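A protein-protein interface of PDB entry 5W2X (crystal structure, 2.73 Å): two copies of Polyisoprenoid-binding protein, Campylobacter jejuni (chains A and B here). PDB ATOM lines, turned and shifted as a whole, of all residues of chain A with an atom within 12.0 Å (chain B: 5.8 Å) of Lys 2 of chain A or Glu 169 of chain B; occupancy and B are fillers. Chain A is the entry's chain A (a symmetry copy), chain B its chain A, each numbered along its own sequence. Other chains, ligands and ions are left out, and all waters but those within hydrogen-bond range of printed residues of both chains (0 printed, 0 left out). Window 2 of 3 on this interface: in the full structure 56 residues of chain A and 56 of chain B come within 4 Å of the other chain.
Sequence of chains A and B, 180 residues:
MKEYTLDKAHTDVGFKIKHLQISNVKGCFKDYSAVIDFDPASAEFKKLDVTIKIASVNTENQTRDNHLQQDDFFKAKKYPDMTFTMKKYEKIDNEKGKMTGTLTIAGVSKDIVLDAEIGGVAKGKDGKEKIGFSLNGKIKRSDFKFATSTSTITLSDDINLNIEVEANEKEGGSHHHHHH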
ATOM      1  N   MET A   1       5.130  20.885   8.184  1.00  0.00           N
ATOM      2  CA  MET A   1       6.566  21.059   8.559  1.00  0.00           C
ATOM      3  C   MET A   1       6.730  21.711   9.957  1.00  0.00           C
ATOM      4  O   MET A   1       5.955  22.546  10.346  1.00  0.00           O
ATOM      5  CB  MET A   1       7.298  21.799   7.423  1.00  0.00           C
ATOM      6  CG  MET A   1       8.807  21.889   7.565  1.00  0.00           C
ATOM      7  SD  MET A   1       9.326  23.229   8.675  1.00  0.00           S
ATOM      8  CE  MET A   1       9.129  24.678   7.618  1.00  0.00           C
ATOM      9  N   LYS A   2       7.743  21.292  10.703  1.00  0.00           N
ATOM     10  CA  LYS A   2       8.038  21.781  12.049  1.00  0.00           C
ATOM     11  C   LYS A   2       9.540  21.654  12.290  1.00  0.00           C
ATOM     12  O   LYS A   2      10.198  20.772  11.737  1.00  0.00           O
ATOM     13  CB  LYS A   2       7.285  20.973  13.097  1.00  0.00           C
ATOM     14  CG  LYS A   2       6.001  21.603  13.543  1.00  0.00           C
ATOM     15  CD  LYS A   2       5.114  20.582  14.241  1.00  0.00           C
ATOM     16  CE  LYS A   2       4.281  21.164  15.395  1.00  0.00           C
ATOM     17  NZ  LYS A   2       3.624  22.490  15.157  1.00  0.00           N
ATOM     18  N   GLU A   3      10.072  22.520  13.143  1.00  0.00           N
ATOM     19  CA  GLU A   3      11.516  22.636  13.342  1.00  0.00           C
ATOM     20  C   GLU A   3      11.902  22.052  14.678  1.00  0.00           C
ATOM     21  O   GLU A   3      11.195  22.238  15.678  1.00  0.00           O
ATOM     22  CB  GLU A   3      11.961  24.094  13.255  1.00  0.00           C
ATOM     23  CG  GLU A   3      11.521  24.786  11.967  1.00  0.00           C
ATOM     24  CD  GLU A   3      12.024  26.212  11.840  1.00  0.00           C
ATOM     25  OE1 GLU A   3      11.348  27.008  11.157  1.00  0.00           O
ATOM     26  OE2 GLU A   3      13.095  26.530  12.409  1.00  0.00           O
ATOM     27  N   TYR A   4      13.010  21.317  14.693  1.00  0.00           N
ATOM     28  CA  TYR A   4      13.444  20.658  15.931  1.00  0.00           C
ATOM     29  C   TYR A   4      14.867  21.045  16.298  1.00  0.00           C
ATOM     30  O   TYR A   4      15.589  21.606  15.468  1.00  0.00           O
ATOM     31  CB  TYR A   4      13.302  19.140  15.823  1.00  0.00           C
ATOM     32  CG  TYR A   4      11.894  18.644  15.527  1.00  0.00           C
ATOM     33  CD1 TYR A   4      11.237  18.927  14.272  1.00  0.00           C
ATOM     34  CD2 TYR A   4      11.219  17.851  16.477  1.00  0.00           C
ATOM     35  CE1 TYR A   4       9.948  18.451  14.005  1.00  0.00           C
ATOM     36  CE2 TYR A   4       9.936  17.356  16.213  1.00  0.00           C
ATOM     37  CZ  TYR A   4       9.302  17.652  14.990  1.00  0.00           C
ATOM     38  OH  TYR A   4       8.033  17.139  14.792  1.00  0.00           O
ATOM     39  N   THR A   5      15.246  20.762  17.540  1.00  0.00           N
ATOM     40  CA  THR A   5      16.582  21.033  18.036  1.00  0.00           C
ATOM     41  C   THR A   5      17.014  19.748  18.673  1.00  0.00           C
ATOM     42  O   THR A   5      16.308  19.225  19.546  1.00  0.00           O
ATOM     43  CB  THR A   5      16.586  22.168  19.107  1.00  0.00           C
ATOM     44  OG1 THR A   5      16.100  23.384  18.523  1.00  0.00           O
ATOM     45  CG2 THR A   5      18.006  22.422  19.694  1.00  0.00           C
ATOM     46  N   LEU A   6      18.177  19.244  18.271  1.00  0.00           N
ATOM     47  CA  LEU A   6      18.714  18.026  18.901  1.00  0.00           C
ATOM     48  C   LEU A   6      18.738  18.144  20.411  1.00  0.00           C
ATOM     49  O   LEU A   6      18.947  19.227  20.939  1.00  0.00           O
ATOM     50  CB  LEU A   6      20.134  17.745  18.441  1.00  0.00           C
ATOM     51  CG  LEU A   6      20.396  17.657  16.956  1.00  0.00           C
ATOM     52  CD1 LEU A   6      21.024  18.951  16.450  1.00  0.00           C
ATOM     53  CD2 LEU A   6      21.337  16.498  16.834  1.00  0.00           C
ATOM     54  N   ASP A   7      18.481  17.042  21.098  1.00  0.00           N
ATOM     55  CA  ASP A   7      18.789  16.934  22.512  1.00  0.00           C
ATOM     56  C   ASP A   7      20.123  16.203  22.508  1.00  0.00           C
ATOM     57  O   ASP A   7      20.166  14.980  22.365  1.00  0.00           O
ATOM     58  CB  ASP A   7      17.669  16.184  23.279  1.00  0.00           C
ATOM     59  CG  ASP A   7      18.101  15.669  24.688  1.00  0.00           C
ATOM     60  OD1 ASP A   7      19.160  16.101  25.227  1.00  0.00           O
ATOM     61  OD2 ASP A   7      17.360  14.816  25.258  1.00  0.00           O
ATOM     62  N   LYS A   8      21.209  16.967  22.639  1.00  0.00           N
ATOM     63  CA  LYS A   8      22.577  16.425  22.585  1.00  0.00           C
ATOM     64  C   LYS A   8      22.826  15.304  23.614  1.00  0.00           C
ATOM     65  O   LYS A   8      23.670  14.420  23.382  1.00  0.00           O
ATOM     66  CB  LYS A   8      23.640  17.539  22.707  1.00  0.00           C
ATOM     67  CG  LYS A   8      23.855  18.433  21.475  1.00  0.00           C
ATOM     68  CD  LYS A   8      25.348  18.735  21.254  1.00  0.00           C
ATOM     69  CE  LYS A   8      25.674  20.180  20.867  1.00  0.00           C
ATOM     70  NZ  LYS A   8      25.058  20.647  19.591  1.00  0.00           N
ATOM     71  N   THR A  11      21.362  12.012  22.025  1.00  0.00           N
ATOM     72  CA  THR A  11      21.766  11.874  20.630  1.00  0.00           C
ATOM     73  C   THR A  11      23.204  11.342  20.609  1.00  0.00           C
ATOM     74  O   THR A  11      24.051  11.774  21.398  1.00  0.00           O
ATOM     75  CB  THR A  11      21.614  13.213  19.848  1.00  0.00           C
ATOM     76  OG1 THR A  11      20.229  13.482  19.588  1.00  0.00           O
ATOM     77  CG2 THR A  11      22.340  13.180  18.523  1.00  0.00           C
ATOM     78  N   ILE B  36      16.951  20.533  11.801  1.00  0.00           N
ATOM     79  CA  ILE B  36      15.979  19.474  11.535  1.00  0.00           C
ATOM     80  C   ILE B  36      14.527  19.957  11.258  1.00  0.00           C
ATOM     81  O   ILE B  36      13.821  20.425  12.169  1.00  0.00           O
ATOM     82  CB  ILE B  36      15.992  18.438  12.667  1.00  0.00           C
ATOM     83  CG1 ILE B  36      17.424  18.153  13.121  1.00  0.00           C
ATOM     84  CG2 ILE B  36      15.317  17.167  12.180  1.00  0.00           C
ATOM     85  CD1 ILE B  36      17.530  17.348  14.409  1.00  0.00           C
ATOM     86  N   ASP B  37      14.100  19.820  10.001  1.00  0.00           N
ATOM     87  CA  ASP B  37      12.723  20.098   9.573  1.00  0.00           C
ATOM     88  C   ASP B  37      11.959  18.834   9.233  1.00  0.00           C
ATOM     89  O   ASP B  37      12.287  18.130   8.249  1.00  0.00           O
ATOM     90  CB  ASP B  37      12.700  20.980   8.337  1.00  0.00           C
ATOM     91  CG  ASP B  37      13.123  22.410   8.621  1.00  0.00           C
ATOM     92  OD1 ASP B  37      13.504  22.727   9.797  1.00  0.00           O
ATOM     93  OD2 ASP B  37      13.061  23.211   7.635  1.00  0.00           O
ATOM     94  N   PHE B  38      10.912  18.588  10.020  1.00  0.00           N
ATOM     95  CA  PHE B  38      10.152  17.355   9.937  1.00  0.00           C
ATOM     96  C   PHE B  38       8.651  17.566  10.107  1.00  0.00           C
ATOM     97  O   PHE B  38       8.215  18.212  11.053  1.00  0.00           O
ATOM     98  CB  PHE B  38      10.686  16.371  10.994  1.00  0.00           C
ATOM     99  CG  PHE B  38      10.034  15.031  10.953  1.00  0.00           C
ATOM    100  CD1 PHE B  38      10.309  14.139   9.910  1.00  0.00           C
ATOM    101  CD2 PHE B  38       9.126  14.656  11.952  1.00  0.00           C
ATOM    102  CE1 PHE B  38       9.681  12.892   9.874  1.00  0.00           C
ATOM    103  CE2 PHE B  38       8.495  13.415  11.917  1.00  0.00           C
ATOM    104  CZ  PHE B  38       8.776  12.530  10.878  1.00  0.00           C
ATOM    105  N   ASP B  39       7.872  16.965   9.215  1.00  0.00           N
ATOM    106  CA  ASP B  39       6.408  17.084   9.206  1.00  0.00           C
ATOM    107  C   ASP B  39       5.689  15.868   9.765  1.00  0.00           C
ATOM    108  O   ASP B  39       5.373  14.948   8.991  1.00  0.00           O
ATOM    109  CB  ASP B  39       5.890  17.349   7.780  1.00  0.00           C
ATOM    110  CG  ASP B  39       4.392  17.581   7.729  1.00  0.00           C
ATOM    111  OD1 ASP B  39       3.763  17.919   8.771  1.00  0.00           O
ATOM    112  OD2 ASP B  39       3.843  17.421   6.628  1.00  0.00           O
ATOM    113  N   PRO B  40       5.333  15.894  11.071  1.00  0.00           N
ATOM    114  CA  PRO B  40       4.651  14.738  11.666  1.00  0.00           C
ATOM    115  C   PRO B  40       3.303  14.375  11.022  1.00  0.00           C
ATOM    116  O   PRO B  40       2.871  13.235  11.135  1.00  0.00           O
ATOM    117  CB  PRO B  40       4.471  15.141  13.134  1.00  0.00           C
ATOM    118  CG  PRO B  40       5.311  16.359  13.318  1.00  0.00           C
ATOM    119  CD  PRO B  40       5.309  17.037  11.992  1.00  0.00           C
ATOM    120  N   GLY B 127       3.244  19.615  26.109  1.00  0.00           N
ATOM    121  CA  GLY B 127       2.481  19.820  24.862  1.00  0.00           C
ATOM    122  C   GLY B 127       3.250  20.282  23.610  1.00  0.00           C
ATOM    123  O   GLY B 127       2.644  20.508  22.553  1.00  0.00           O
ATOM    124  N   LYS B 128       4.575  20.431  23.721  1.00  0.00           N
ATOM    125  CA  LYS B 128       5.463  20.688  22.569  1.00  0.00           C
ATOM    126  C   LYS B 128       6.029  19.374  22.010  1.00  0.00           C
ATOM    127  O   LYS B 128       6.280  18.420  22.762  1.00  0.00           O
ATOM    128  CB  LYS B 128       6.602  21.633  22.964  1.00  0.00           C
ATOM    129  CG  LYS B 128       6.304  23.111  22.752  1.00  0.00           C
ATOM    130  CD  LYS B 128       6.542  23.925  24.023  1.00  0.00           C
ATOM    131  CE  LYS B 128       7.995  24.329  24.232  1.00  0.00           C
ATOM    132  NZ  LYS B 128       8.320  25.570  23.477  1.00  0.00           N
ATOM    133  N   GLU B 129       6.249  19.352  20.695  1.00  0.00           N
ATOM    134  CA  GLU B 129       6.661  18.146  19.943  1.00  0.00           C
ATOM    135  C   GLU B 129       8.024  17.528  20.295  1.00  0.00           C
ATOM    136  O   GLU B 129       8.975  18.230  20.686  1.00  0.00           O
ATOM    137  CB  GLU B 129       6.655  18.445  18.440  1.00  0.00           C
ATOM    138  CG  GLU B 129       5.288  18.715  17.836  1.00  0.00           C
ATOM    139  CD  GLU B 129       4.640  17.494  17.220  1.00  0.00           C
ATOM    140  OE1 GLU B 129       3.465  17.647  16.843  1.00  0.00           O
ATOM    141  OE2 GLU B 129       5.285  16.413  17.094  1.00  0.00           O
ATOM    142  N   LYS B 130       8.091  16.209  20.135  1.00  0.00           N
ATOM    143  CA  LYS B 130       9.359  15.491  20.088  1.00  0.00           C
ATOM    144  C   LYS B 130       9.366  14.455  18.968  1.00  0.00           C
ATOM    145  O   LYS B 130       8.300  14.148  18.414  1.00  0.00           O
ATOM    146  CB  LYS B 130       9.748  14.897  21.453  1.00  0.00           C
ATOM    147  CG  LYS B 130       8.660  14.159  22.206  1.00  0.00           C
ATOM    148  CD  LYS B 130       9.084  13.888  23.645  1.00  0.00           C
ATOM    149  CE  LYS B 130       8.133  12.908  24.324  1.00  0.00           C
ATOM    150  NZ  LYS B 130       8.869  11.928  25.182  1.00  0.00           N
ATOM    151  N   ALA B 167      15.067  14.583  19.770  1.00  0.00           N
ATOM    152  CA  ALA B 167      14.952  15.994  19.355  1.00  0.00           C
ATOM    153  C   ALA B 167      13.568  16.624  19.623  1.00  0.00           C
ATOM    154  O   ALA B 167      12.527  16.006  19.356  1.00  0.00           O
ATOM    155  CB  ALA B 167      15.342  16.167  17.891  1.00  0.00           C
ATOM    156  N   ASN B 168      13.588  17.869  20.112  1.00  0.00           N
ATOM    157  CA  ASN B 168      12.405  18.601  20.569  1.00  0.00           C
ATOM    158  C   ASN B 168      12.147  19.805  19.686  1.00  0.00           C
ATOM    159  O   ASN B 168      13.047  20.279  18.993  1.00  0.00           O
ATOM    160  CB  ASN B 168      12.606  19.039  22.011  1.00  0.00           C
ATOM    161  CG  ASN B 168      12.982  17.877  22.930  1.00  0.00           C
ATOM    162  OD1 ASN B 168      12.127  17.080  23.340  1.00  0.00           O
ATOM    163  ND2 ASN B 168      14.269  17.773  23.255  1.00  0.00           N
ATOM    164  N   GLU B 169      10.911  20.287  19.702  1.00  0.00           N
ATOM    165  CA  GLU B 169      10.510  21.395  18.849  1.00  0.00           C
ATOM    166  C   GLU B 169      11.229  22.714  19.235  1.00  0.00           C
ATOM    167  O   GLU B 169      11.903  22.773  20.262  1.00  0.00           O
ATOM    168  CB  GLU B 169       8.996  21.533  18.914  1.00  0.00           C
ATOM    169  CG  GLU B 169       8.368  22.089  17.648  1.00  0.00           C
ATOM    170  CD  GLU B 169       6.877  22.387  17.786  1.00  0.00           C
ATOM    171  OE1 GLU B 169       6.331  23.039  16.861  1.00  0.00           O
ATOM    172  OE2 GLU B 169       6.246  21.974  18.798  1.00  0.00           O
ATOM    173  N   LYS B 170      11.070  23.762  18.420  1.00  0.00           N
ATOM    174  CA  LYS B 170      11.846  25.008  18.532  1.00  0.00           C
ATOM    175  C   LYS B 170      11.072  26.200  19.163  1.00  0.00           C
ATOM    176  O   LYS B 170       9.841  26.148  19.275  1.00  0.00           O
ATOM    177  CB  LYS B 170      12.379  25.386  17.138  1.00  0.00           C
ATOM    178  CG  LYS B 170      13.897  25.573  17.094  1.00  0.00           C
ATOM    179  CD  LYS B 170      14.303  26.554  15.991  1.00  0.00           C
ATOM    180  CE  LYS B 170      15.688  27.159  16.392  1.00  0.00           C
ATOM    181  NZ  LYS B 170      16.109  28.285  15.485  1.00  0.00           N
ATOM    182  N   GLU B 171      11.812  27.258  19.550  1.00  0.00           N
ATOM    183  CA  GLU B 171      11.305  28.523  20.170  1.00  0.00           C
ATOM    184  C   GLU B 171      10.558  28.285  21.483  1.00  0.00           C
ATOM    185  O   GLU B 171      10.969  27.449  22.294  1.00  0.00           O
ATOM    186  CB  GLU B 171      10.470  29.390  19.194  1.00  0.00           C
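The backbone NH (N) of Phe 38 of chain B is in hydrogen-bond range of the backbone carbonyl oxygen (O) of Lys 2 of chain A. The backbone NH (N) of Tyr 4 of chain A sits at hydrogen-bond distance from the backbone carbonyl oxygen (O) of Ile 36 of chain B (2.8 Å). The side-chain carboxylate (OE1) of Glu 169 of chain B lies within salt-bridge range of the side-chain amino group (NZ) of Lys 2 of chain A, 3.2 Å away. O of Glu 3 of chain A is in hydrogen-bond range of N of Lys 170 of chain B (3.1 Å). O of Asn 168 of chain B sits at hydrogen-bond distance from N of Thr 5 of chain A (2.7 Å). The side-chain carboxylate (OD1) of Asp 39 of chain B lies within hydrogen-bond range of the backbone NH (N) of Met 1 of chain A, at 3.3 Å.
N of Glu 169 of chain B lies within hydrogen-bond range of O of Glu 129 of chain B, at 3.0 Å. The backbone carbonyl oxygen (O) of Asp 7 of chain A sits at hydrogen-bond distance from the side-chain hydroxyl (OG1) of Thr 11 of chain A (3.2 Å).
OD2 of Asp 37 of chain B touches SD of Met 1 of chain A, 3.9 Å away. O of Phe 38 of chain B touches C of Met 1 of chain A, 3.96 Å away. CE of Lys 2 of chain A touches CG of Glu 129 of chain B, at 3.6 Å. CG of Glu 3 of chain A touches OD1 of Asp 37 of chain B, 3.6 Å away. Tyr 4 of chain A touches Phe 38 of chain B (CE1 to O, 3.4 Å). CG of Pro 40 of chain B touches OH of Tyr 4 of chain A (3.2 Å). Tyr 4 of chain A touches Glu 129 of chain B. Tyr 4 of chain A touches Asn 168 of chain B (CA to O, 3.1 Å). Ala 167 of chain B touches Thr 5 of chain A (CA to O, 3.5 Å). Leu 6 of chain A touches Ile 36 of chain B (CG to CD1, 3.8 Å).
Of chain B, only Ile 36 (3.7 Å), Asp 37 (3.4 Å), Phe 38 (2.9 Å), Glu 129 (3.6 Å) and Glu 169 (3.1 Å) come within 4 Å of Lys 2 of chain A. Printed residues of chain B within 4 Å of Tyr 4 of chain A: Ile 36, Phe 38, Pro 40, Glu 129, Ala 167 and Asn 168. Printed residues of chain B within 4 Å of Thr 5 of chain A: Ala 167, Asn 168 and Lys 170. Of the printed residues of chain B, Leu 6 of chain A touches Ile 36 (3.8 Å) and Ala 167 (3.98 Å). Printed residues of chain B within 4 Å of Asp 7 of chain A: Asn 168 (3.8 Å). Asp 37 of chain B touches just these residues of chain A: Met 1 (3.9 Å), Lys 2 (3.4 Å) and Glu 3 (3.6 Å). Printed residues of chain A within 4 Å of Phe 38 of chain B: Met 1, Lys 2 and Tyr 4. Asp 39 of chain B touches one residue of chain A. Of chain A, only Lys 2 and Tyr 4 come within 4 Å of Glu 129 of chain B. Glu 171 of chain B touches none of the printed residues of chain A. The nearest residue of chain B that does not touch Lys 2 of chain A is Pro 40 of chain B (4.2 Å).
Of the 9 printed residues of chain A, 7 touch a printed residue of chain B. Hydrophobic or aromatic side chains of chain A that line the printed part of chain B: Met 1, Tyr 4 and Leu 6. Among the printed residues, 24 pairs touch across the chains. Among the printed residues, Asp or Glu carboxylates within 4 Å of a Lys or Arg side-chain nitrogen of the other chain: Lys 2 of chain A with Glu 169 of chain B (3.2 Å).
No position is printed for both chains. Of the 24 pairs that touch across the chains among the printed residues, none has its exchanged pair printed and touching as well.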
